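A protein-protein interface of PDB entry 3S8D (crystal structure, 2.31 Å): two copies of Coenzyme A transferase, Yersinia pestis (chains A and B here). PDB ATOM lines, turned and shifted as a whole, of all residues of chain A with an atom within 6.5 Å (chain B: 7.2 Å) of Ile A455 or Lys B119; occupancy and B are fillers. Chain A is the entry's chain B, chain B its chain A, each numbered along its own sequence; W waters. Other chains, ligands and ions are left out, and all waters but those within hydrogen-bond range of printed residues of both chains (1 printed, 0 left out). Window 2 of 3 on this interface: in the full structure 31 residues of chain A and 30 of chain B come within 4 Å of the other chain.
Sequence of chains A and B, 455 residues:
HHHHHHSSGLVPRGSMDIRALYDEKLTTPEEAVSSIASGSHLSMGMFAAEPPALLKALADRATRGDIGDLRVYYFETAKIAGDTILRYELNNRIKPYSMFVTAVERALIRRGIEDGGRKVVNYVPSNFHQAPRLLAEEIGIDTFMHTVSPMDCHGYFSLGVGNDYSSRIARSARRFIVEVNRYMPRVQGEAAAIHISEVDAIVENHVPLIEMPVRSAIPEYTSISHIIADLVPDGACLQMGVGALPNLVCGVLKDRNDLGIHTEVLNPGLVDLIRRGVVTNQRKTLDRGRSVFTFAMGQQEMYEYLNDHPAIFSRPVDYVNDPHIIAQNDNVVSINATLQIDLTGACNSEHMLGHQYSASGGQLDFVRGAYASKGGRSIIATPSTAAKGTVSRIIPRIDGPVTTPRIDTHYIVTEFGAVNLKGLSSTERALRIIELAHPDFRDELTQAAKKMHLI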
ATOM      1  N   SER A 425      -8.543  -8.488   9.936  1.00  0.00           N
ATOM      2  CA  SER A 425      -8.917  -9.851  10.317  1.00  0.00           C
ATOM      3  C   SER A 425      -8.141 -10.866   9.470  1.00  0.00           C
ATOM      4  O   SER A 425      -7.490 -10.517   8.481  1.00  0.00           O
ATOM      5  CB  SER A 425     -10.415 -10.074  10.134  1.00  0.00           C
ATOM      6  OG  SER A 425     -10.761  -9.985   8.764  1.00  0.00           O
ATOM      7  N   SER A 426      -8.201 -12.127   9.867  1.00  0.00           N
ATOM      8  CA  SER A 426      -7.635 -13.186   9.058  1.00  0.00           C
ATOM      9  C   SER A 426      -8.167 -13.146   7.628  1.00  0.00           C
ATOM     10  O   SER A 426      -7.413 -13.309   6.669  1.00  0.00           O
ATOM     11  CB  SER A 426      -7.946 -14.533   9.701  1.00  0.00           C
ATOM     12  OG  SER A 426      -6.987 -14.823  10.694  1.00  0.00           O
ATOM     13  N   THR A 427      -9.468 -12.933   7.486  1.00  0.00           N
ATOM     14  CA  THR A 427     -10.095 -12.833   6.170  1.00  0.00           C
ATOM     15  C   THR A 427      -9.550 -11.666   5.330  1.00  0.00           C
ATOM     16  O   THR A 427      -9.125 -11.852   4.178  1.00  0.00           O
ATOM     17  CB  THR A 427     -11.632 -12.713   6.284  1.00  0.00           C
ATOM     18  OG1 THR A 427     -12.192 -14.011   6.525  1.00  0.00           O
ATOM     19  CG2 THR A 427     -12.230 -12.131   4.995  1.00  0.00           C
ATOM     20  N   GLU A 428      -9.589 -10.463   5.886  1.00  0.00           N
ATOM     21  CA  GLU A 428      -9.067  -9.313   5.169  1.00  0.00           C
ATOM     22  C   GLU A 428      -7.600  -9.521   4.785  1.00  0.00           C
ATOM     23  O   GLU A 428      -7.165  -9.074   3.729  1.00  0.00           O
ATOM     24  CB  GLU A 428      -9.193  -8.061   6.024  1.00  0.00           C
ATOM     25  CG  GLU A 428     -10.625  -7.665   6.327  1.00  0.00           C
ATOM     26  CD  GLU A 428     -10.713  -6.749   7.539  1.00  0.00           C
ATOM     27  OE1 GLU A 428      -9.911  -6.945   8.489  1.00  0.00           O
ATOM     28  OE2 GLU A 428     -11.579  -5.844   7.542  1.00  0.00           O
ATOM     29  N   ALA A 430      -6.093 -12.543   4.240  1.00  0.00           N
ATOM     30  CA  ALA A 430      -6.064 -13.528   3.165  1.00  0.00           C
ATOM     31  C   ALA A 430      -6.415 -12.869   1.838  1.00  0.00           C
ATOM     32  O   ALA A 430      -5.695 -13.022   0.854  1.00  0.00           O
ATOM     33  CB  ALA A 430      -7.012 -14.710   3.462  1.00  0.00           C
ATOM     34  N   LEU A 431      -7.509 -12.112   1.825  1.00  0.00           N
ATOM     35  CA  LEU A 431      -8.001 -11.521   0.593  1.00  0.00           C
ATOM     36  C   LEU A 431      -7.026 -10.514   0.024  1.00  0.00           C
ATOM     37  O   LEU A 431      -6.840 -10.459  -1.177  1.00  0.00           O
ATOM     38  CB  LEU A 431      -9.378 -10.877   0.783  1.00  0.00           C
ATOM     39  CG  LEU A 431     -10.509 -11.761   1.312  1.00  0.00           C
ATOM     40  CD1 LEU A 431     -11.774 -10.936   1.571  1.00  0.00           C
ATOM     41  CD2 LEU A 431     -10.815 -12.938   0.387  1.00  0.00           C
ATOM     42  N   ILE A 434      -3.604 -12.469  -1.132  1.00  0.00           N
ATOM     43  CA  ILE A 434      -3.887 -13.134  -2.395  1.00  0.00           C
ATOM     44  C   ILE A 434      -3.700 -12.188  -3.602  1.00  0.00           C
ATOM     45  O   ILE A 434      -3.071 -12.566  -4.597  1.00  0.00           O
ATOM     46  CB  ILE A 434      -5.301 -13.743  -2.388  1.00  0.00           C
ATOM     47  CG1 ILE A 434      -5.356 -14.918  -1.396  1.00  0.00           C
ATOM     48  CG2 ILE A 434      -5.702 -14.168  -3.797  1.00  0.00           C
ATOM     49  CD1 ILE A 434      -6.716 -15.585  -1.268  1.00  0.00           C
ATOM     50  N   THR A 446      -7.016 -18.854  -3.287  1.00  0.00           N
ATOM     51  CA  THR A 446      -8.372 -18.601  -2.811  1.00  0.00           C
ATOM     52  C   THR A 446      -9.066 -19.868  -2.339  1.00  0.00           C
ATOM     53  O   THR A 446      -9.827 -19.829  -1.368  1.00  0.00           O
ATOM     54  CB  THR A 446      -9.232 -17.916  -3.867  1.00  0.00           C
ATOM     55  OG1 THR A 446      -8.631 -16.665  -4.208  1.00  0.00           O
ATOM     56  CG2 THR A 446     -10.646 -17.671  -3.339  1.00  0.00           C
ATOM     57  N   ALA A 449      -7.590 -20.859   1.010  1.00  0.00           N
ATOM     58  CA  ALA A 449      -8.086 -19.996   2.085  1.00  0.00           C
ATOM     59  C   ALA A 449      -9.340 -20.538   2.755  1.00  0.00           C
ATOM     60  O   ALA A 449      -9.535 -20.353   3.950  1.00  0.00           O
ATOM     61  CB  ALA A 449      -8.342 -18.582   1.578  1.00  0.00           C
ATOM     62  N   LYS A 450     -10.197 -21.175   1.963  1.00  0.00           N
ATOM     63  CA  LYS A 450     -11.459 -21.704   2.457  1.00  0.00           C
ATOM     64  C   LYS A 450     -11.248 -23.039   3.155  1.00  0.00           C
ATOM     65  O   LYS A 450     -11.963 -23.379   4.096  1.00  0.00           O
ATOM     66  CB  LYS A 450     -12.460 -21.862   1.313  1.00  0.00           C
ATOM     67  CG  LYS A 450     -12.879 -20.551   0.671  1.00  0.00           C
ATOM     68  CD  LYS A 450     -13.871 -20.783  -0.455  1.00  0.00           C
ATOM     69  CE  LYS A 450     -14.254 -19.476  -1.130  1.00  0.00           C
ATOM     70  NZ  LYS A 450     -14.948 -18.550  -0.196  1.00  0.00           N
ATOM     71  N   LYS A 451     -10.260 -23.795   2.689  1.00  0.00           N
ATOM     72  CA  LYS A 451      -9.929 -25.073   3.313  1.00  0.00           C
ATOM     73  C   LYS A 451      -9.413 -24.817   4.729  1.00  0.00           C
ATOM     74  O   LYS A 451      -9.644 -25.619   5.633  1.00  0.00           O
ATOM     75  CB  LYS A 451      -8.837 -25.787   2.527  1.00  0.00           C
ATOM     76  CG  LYS A 451      -9.154 -25.992   1.049  1.00  0.00           C
ATOM     77  CD  LYS A 451     -10.191 -27.090   0.839  1.00  0.00           C
ATOM     78  CE  LYS A 451     -10.892 -26.951  -0.516  1.00  0.00           C
ATOM     79  NZ  LYS A 451      -9.958 -27.090  -1.682  1.00  0.00           N
ATOM     80  N   MET A 452      -8.725 -23.687   4.911  1.00  0.00           N
ATOM     81  CA  MET A 452      -8.164 -23.314   6.204  1.00  0.00           C
ATOM     82  C   MET A 452      -9.160 -22.391   6.905  1.00  0.00           C
ATOM     83  O   MET A 452      -8.903 -21.890   8.017  1.00  0.00           O
ATOM     84  CB  MET A 452      -6.820 -22.613   6.027  1.00  0.00           C
ATOM     85  CG  MET A 452      -5.827 -23.353   5.133  1.00  0.00           C
ATOM     86  SD  MET A 452      -4.440 -22.285   4.648  1.00  0.00           S
ATOM     87  CE  MET A 452      -3.087 -23.463   4.741  1.00  0.00           C
ATOM     88  N   HIS A 453     -10.295 -22.173   6.234  1.00  0.00           N
ATOM     89  CA  HIS A 453     -11.414 -21.374   6.758  1.00  0.00           C
ATOM     90  C   HIS A 453     -11.052 -19.918   7.049  1.00  0.00           C
ATOM     91  O   HIS A 453     -11.755 -19.245   7.801  1.00  0.00           O
ATOM     92  CB  HIS A 453     -12.041 -22.037   7.999  1.00  0.00           C
ATOM     93  CG  HIS A 453     -12.590 -23.409   7.741  1.00  0.00           C
ATOM     94  ND1 HIS A 453     -13.707 -23.635   6.959  1.00  0.00           N
ATOM     95  CD2 HIS A 453     -12.169 -24.631   8.158  1.00  0.00           C
ATOM     96  CE1 HIS A 453     -13.947 -24.935   6.905  1.00  0.00           C
ATOM     97  NE2 HIS A 453     -13.030 -25.561   7.625  1.00  0.00           N
ATOM     98  N   LEU A 454      -9.958 -19.441   6.457  1.00  0.00           N
ATOM     99  CA  LEU A 454      -9.625 -18.022   6.493  1.00  0.00           C
ATOM    100  C   LEU A 454     -10.666 -17.230   5.715  1.00  0.00           C
ATOM    101  O   LEU A 454     -10.856 -16.033   5.941  1.00  0.00           O
ATOM    102  CB  LEU A 454      -8.273 -17.776   5.844  1.00  0.00           C
ATOM    103  CG  LEU A 454      -7.042 -18.376   6.498  1.00  0.00           C
ATOM    104  CD1 LEU A 454      -5.825 -17.928   5.716  1.00  0.00           C
ATOM    105  CD2 LEU A 454      -6.945 -17.947   7.970  1.00  0.00           C
ATOM    106  N   ILE A 455     -11.335 -17.926   4.800  1.00  0.00           N
ATOM    107  CA  ILE A 455     -12.210 -17.330   3.779  1.00  0.00           C
ATOM    108  C   ILE A 455     -11.671 -16.046   3.149  1.00  0.00           C
ATOM    109  O   ILE A 455     -10.545 -16.016   2.641  1.00  0.00           O
ATOM    110  CB  ILE A 455     -13.642 -17.100   4.289  1.00  0.00           C
ATOM    111  CG1 ILE A 455     -14.283 -18.429   4.685  1.00  0.00           C
ATOM    112  CG2 ILE A 455     -14.478 -16.431   3.209  1.00  0.00           C
ATOM    113  CD1 ILE A 455     -15.805 -18.356   4.774  1.00  0.00           C
ATOM    114  N   TYR B  88     -24.640 -17.061  19.101  1.00  0.00           N
ATOM    115  CA  TYR B  88     -24.516 -17.537  17.724  1.00  0.00           C
ATOM    116  C   TYR B  88     -25.598 -17.001  16.768  1.00  0.00           C
ATOM    117  O   TYR B  88     -25.308 -16.695  15.606  1.00  0.00           O
ATOM    118  CB  TYR B  88     -24.492 -19.070  17.700  1.00  0.00           C
ATOM    119  CG  TYR B  88     -24.178 -19.637  16.337  1.00  0.00           C
ATOM    120  CD1 TYR B  88     -22.867 -19.688  15.871  1.00  0.00           C
ATOM    121  CD2 TYR B  88     -25.191 -20.114  15.508  1.00  0.00           C
ATOM    122  CE1 TYR B  88     -22.571 -20.197  14.618  1.00  0.00           C
ATOM    123  CE2 TYR B  88     -24.905 -20.626  14.253  1.00  0.00           C
ATOM    124  CZ  TYR B  88     -23.595 -20.663  13.813  1.00  0.00           C
ATOM    125  OH  TYR B  88     -23.305 -21.172  12.567  1.00  0.00           O
ATOM    126  N   ASN B  91     -24.949 -13.656  15.228  1.00  0.00           N
ATOM    127  CA  ASN B  91     -23.720 -13.619  14.439  1.00  0.00           C
ATOM    128  C   ASN B  91     -23.789 -12.841  13.127  1.00  0.00           C
ATOM    129  O   ASN B  91     -22.862 -12.108  12.789  1.00  0.00           O
ATOM    130  CB  ASN B  91     -23.228 -15.044  14.169  1.00  0.00           C
ATOM    131  CG  ASN B  91     -21.724 -15.118  14.010  1.00  0.00           C
ATOM    132  OD1 ASN B  91     -21.175 -14.690  12.995  1.00  0.00           O
ATOM    133  ND2 ASN B  91     -21.049 -15.663  15.015  1.00  0.00           N
ATOM    134  N   TYR B  97     -15.020  -9.726  16.194  1.00  0.00           N
ATOM    135  CA  TYR B  97     -13.631  -9.599  15.771  1.00  0.00           C
ATOM    136  C   TYR B  97     -12.770  -9.794  16.998  1.00  0.00           C
ATOM    137  O   TYR B  97     -12.371  -8.829  17.659  1.00  0.00           O
ATOM    138  CB  TYR B  97     -13.388  -8.242  15.110  1.00  0.00           C
ATOM    139  CG  TYR B  97     -13.841  -8.251  13.675  1.00  0.00           C
ATOM    140  CD1 TYR B  97     -15.200  -8.275  13.350  1.00  0.00           C
ATOM    141  CD2 TYR B  97     -12.917  -8.278  12.638  1.00  0.00           C
ATOM    142  CE1 TYR B  97     -15.617  -8.306  12.022  1.00  0.00           C
ATOM    143  CE2 TYR B  97     -13.326  -8.312  11.303  1.00  0.00           C
ATOM    144  CZ  TYR B  97     -14.675  -8.328  11.006  1.00  0.00           C
ATOM    145  OH  TYR B  97     -15.076  -8.361   9.691  1.00  0.00           O
ATOM    146  N   LEU B 108     -18.251 -20.772  19.512  1.00  0.00           N
ATOM    147  CA  LEU B 108     -18.782 -20.197  18.278  1.00  0.00           C
ATOM    148  C   LEU B 108     -18.197 -20.832  17.015  1.00  0.00           C
ATOM    149  O   LEU B 108     -18.931 -21.090  16.062  1.00  0.00           O
ATOM    150  CB  LEU B 108     -18.586 -18.674  18.242  1.00  0.00           C
ATOM    151  CG  LEU B 108     -19.438 -17.809  19.169  1.00  0.00           C
ATOM    152  CD1 LEU B 108     -19.124 -16.340  18.921  1.00  0.00           C
ATOM    153  CD2 LEU B 108     -20.930 -18.089  18.968  1.00  0.00           C
ATOM    154  N   ILE B 109     -16.886 -21.073  16.995  1.00  0.00           N
ATOM    155  CA  ILE B 109     -16.256 -21.650  15.802  1.00  0.00           C
ATOM    156  C   ILE B 109     -16.729 -23.085  15.583  1.00  0.00           C
ATOM    157  O   ILE B 109     -17.093 -23.459  14.461  1.00  0.00           O
ATOM    158  CB  ILE B 109     -14.719 -21.647  15.869  1.00  0.00           C
ATOM    159  CG1 ILE B 109     -14.185 -20.225  16.009  1.00  0.00           C
ATOM    160  CG2 ILE B 109     -14.134 -22.310  14.623  1.00  0.00           C
ATOM    161  CD1 ILE B 109     -12.878 -20.159  16.770  1.00  0.00           C
ATOM    162  N   GLY B 112     -20.021 -23.171  14.329  1.00  0.00           N
ATOM    163  CA  GLY B 112     -20.048 -22.514  13.035  1.00  0.00           C
ATOM    164  C   GLY B 112     -19.696 -23.473  11.919  1.00  0.00           C
ATOM    165  O   GLY B 112     -20.126 -23.304  10.773  1.00  0.00           O
ATOM    166  N   ILE B 113     -18.903 -24.482  12.262  1.00  0.00           N
ATOM    167  CA  ILE B 113     -18.514 -25.523  11.323  1.00  0.00           C
ATOM    168  C   ILE B 113     -19.665 -26.510  11.117  1.00  0.00           C
ATOM    169  O   ILE B 113     -20.094 -26.756   9.983  1.00  0.00           O
ATOM    170  CB  ILE B 113     -17.268 -26.258  11.820  1.00  0.00           C
ATOM    171  CG1 ILE B 113     -16.089 -25.284  11.883  1.00  0.00           C
ATOM    172  CG2 ILE B 113     -16.953 -27.442  10.911  1.00  0.00           C
ATOM    173  CD1 ILE B 113     -14.942 -25.771  12.742  1.00  0.00           C
ATOM    174  N   GLY B 116     -22.613 -25.995   8.090  1.00  0.00           N
ATOM    175  CA  GLY B 116     -22.243 -25.857   6.696  1.00  0.00           C
ATOM    176  C   GLY B 116     -20.960 -25.067   6.560  1.00  0.00           C
ATOM    177  O   GLY B 116     -20.759 -24.338   5.579  1.00  0.00           O
ATOM    178  N   GLY B 117     -20.098 -25.209   7.563  1.00  0.00           N
ATOM    179  CA  GLY B 117     -18.801 -24.560   7.567  1.00  0.00           C
ATOM    180  C   GLY B 117     -18.809 -23.067   7.284  1.00  0.00           C
ATOM    181  O   GLY B 117     -18.002 -22.579   6.487  1.00  0.00           O
ATOM    182  N   ARG B 118     -19.716 -22.330   7.921  1.00  0.00           N
ATOM    183  CA  ARG B 118     -19.656 -20.870   7.857  1.00  0.00           C
ATOM    184  C   ARG B 118     -18.560 -20.338   8.797  1.00  0.00           C
ATOM    185  O   ARG B 118     -18.181 -21.010   9.767  1.00  0.00           O
ATOM    186  CB  ARG B 118     -21.016 -20.249   8.184  1.00  0.00           C
ATOM    187  CG  ARG B 118     -21.701 -20.878   9.375  1.00  0.00           C
ATOM    188  CD  ARG B 118     -23.102 -20.316   9.575  1.00  0.00           C
ATOM    189  NE  ARG B 118     -23.102 -18.856   9.696  1.00  0.00           N
ATOM    190  CZ  ARG B 118     -24.008 -18.150  10.377  1.00  0.00           C
ATOM    191  NH1 ARG B 118     -24.997 -18.769  11.012  1.00  0.00           N
ATOM    192  NH2 ARG B 118     -23.924 -16.822  10.427  1.00  0.00           N
ATOM    193  N   LYS B 119     -18.031 -19.155   8.480  1.00  0.00           N
ATOM    194  CA  LYS B 119     -17.000 -18.507   9.297  1.00  0.00           C
ATOM    195  C   LYS B 119     -17.660 -17.448  10.176  1.00  0.00           C
ATOM    196  O   LYS B 119     -18.120 -16.410   9.683  1.00  0.00           O
ATOM    197  CB  LYS B 119     -15.935 -17.857   8.404  1.00  0.00           C
ATOM    198  CG  LYS B 119     -14.687 -17.341   9.127  1.00  0.00           C
ATOM    199  CD  LYS B 119     -14.113 -16.129   8.390  1.00  0.00           C
ATOM    200  CE  LYS B 119     -14.998 -14.895   8.604  1.00  0.00           C
ATOM    201  NZ  LYS B 119     -14.845 -13.831   7.562  1.00  0.00           N
ATOM    202  N   VAL B 120     -17.703 -17.712  11.480  1.00  0.00           N
ATOM    203  CA  VAL B 120     -18.476 -16.881  12.408  1.00  0.00           C
ATOM    204  C   VAL B 120     -17.611 -15.971  13.301  1.00  0.00           C
ATOM    205  O   VAL B 120     -18.080 -14.937  13.802  1.00  0.00           O
ATOM    206  CB  VAL B 120     -19.441 -17.742  13.278  1.00  0.00           C
ATOM    207  CG1 VAL B 120     -20.612 -18.257  12.441  1.00  0.00           C
ATOM    208  CG2 VAL B 120     -18.696 -18.900  13.953  1.00  0.00           C
ATOM    209  N   VAL B 121     -16.352 -16.354  13.498  1.00  0.00           N
ATOM    210  CA  VAL B 121     -15.413 -15.522  14.245  1.00  0.00           C
ATOM    211  C   VAL B 121     -14.346 -14.930  13.310  1.00  0.00           C
ATOM    212  O   VAL B 121     -13.663 -15.666  12.593  1.00  0.00           O
ATOM    213  CB  VAL B 121     -14.753 -16.329  15.398  1.00  0.00           C
ATOM    214  CG1 VAL B 121     -13.733 -15.482  16.148  1.00  0.00           C
ATOM    215  CG2 VAL B 121     -15.810 -16.857  16.358  1.00  0.00           C
ATOM    216  N   ASN B 122     -14.215 -13.604  13.295  1.00  0.00           N
ATOM    217  CA  ASN B 122     -13.099 -12.962  12.589  1.00  0.00           C
ATOM    218  C   ASN B 122     -11.928 -12.718  13.548  1.00  0.00           C
ATOM    219  O   ASN B 122     -11.983 -11.825  14.388  1.00  0.00           O
ATOM    220  CB  ASN B 122     -13.526 -11.639  11.945  1.00  0.00           C
ATOM    221  CG  ASN B 122     -14.506 -11.833  10.803  1.00  0.00           C
ATOM    222  OD1 ASN B 122     -14.127 -11.802   9.624  1.00  0.00           O
ATOM    223  ND2 ASN B 122     -15.776 -12.039  11.142  1.00  0.00           N
ATOM    224  N   TYR B 123     -10.873 -13.516  13.436  1.00  0.00           N
ATOM    225  CA  TYR B 123      -9.732 -13.340  14.303  1.00  0.00           C
ATOM    226  C   TYR B 123      -8.890 -12.170  13.800  1.00  0.00           C
ATOM    227  O   TYR B 123      -8.546 -12.101  12.615  1.00  0.00           O
ATOM    228  CB  TYR B 123      -8.909 -14.640  14.371  1.00  0.00           C
ATOM    229  CG  TYR B 123      -7.635 -14.554  15.195  1.00  0.00           C
ATOM    230  CD1 TYR B 123      -7.678 -14.339  16.566  1.00  0.00           C
ATOM    231  CD2 TYR B 123      -6.391 -14.704  14.598  1.00  0.00           C
ATOM    232  CE1 TYR B 123      -6.507 -14.267  17.315  1.00  0.00           C
ATOM    233  CE2 TYR B 123      -5.224 -14.632  15.332  1.00  0.00           C
ATOM    234  CZ  TYR B 123      -5.288 -14.419  16.684  1.00  0.00           C
ATOM    235  OH  TYR B 123      -4.120 -14.347  17.405  1.00  0.00           O
HETATM  236  O   HOH W   1     -11.362 -13.493   9.888  1.00  0.00           O
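The side-chain hydroxyl (OG1) of Thr A427 lies within hydrogen-bond range of the side-chain amino group (NZ) of Lys B119 (2.9 Å).
O of Tyr B123 is in hydrogen-bond range of N of Ser A426, at 2.8 Å.
The side-chain amino group (NZ) of Lys B119 lies within hydrogen-bond range of the side-chain amide oxygen (OD1) of Asn B122 (3.0 Å).
OG of Ser A425 lies close to N of Thr A427 (3.5 Å).
N of Ser A425 lies within hydrogen-bond range of OE1 of Glu A428.
OG1 of Thr A427 is in hydrogen-bond range of O of Leu A454, at 2.5 Å.
O of Ala A449 lies within hydrogen-bond range of N of Ile A455 (3.1 Å).
O of Lys A450 is in hydrogen-bond range of ND1 of His A453, 3.4 Å away.
CB of Ser A425 touches CE2 of Tyr B97, at 3.6 Å.
Asn B122 touches Ser A425 (OD1 to OG, 3.9 Å).
O of Tyr B123 touches CA of Ser A425 (3.2 Å).
Lys B119 touches His A453.
Lys B119 touches Ile A455.
Of chain B, only Lys B119 (3.7 Å) comes within 4 Å of Ile A455.
Lys B119 touches three residues of chain A.
Of the printed residues of chain B, Thr A427 touches Lys B119.
Of the printed residues of chain A, Asn B122 touches Ser A425.
Of the printed residues of chain A, Tyr B123 touches Ser A425 and Ser A426.
Of the printed residues of chain B, Ser A425 touches Tyr B97, Asn B122 and Tyr B123.
Ile B109 touches none of the printed residues of chain A.
The nearest residue of chain B that does not touch Ile A455 is Gly B117 (5.1 Å).
Of the 15 printed residues of chain B, 4 touch a printed residue of chain A.
Printed residues of chain B that touch a printed residue of chain A: Tyr B97, Lys B119, Asn B122 and Tyr B123.
Hydrophobic or aromatic side chains of chain B within 4 Å of the printed part of chain A: Tyr B97 and Tyr B123.
Hydrophobic or aromatic side chains of chain A that line the printed part of chain B: Ile A455.
Among the printed residues, 7 pairs touch across the chains.
No position is printed for both chains.
Water W1 lies within hydrogen-bond range of the backbone NH of Thr A427, the side-chain amide oxygen of Asn B122 and the backbone NH of Ser A426.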
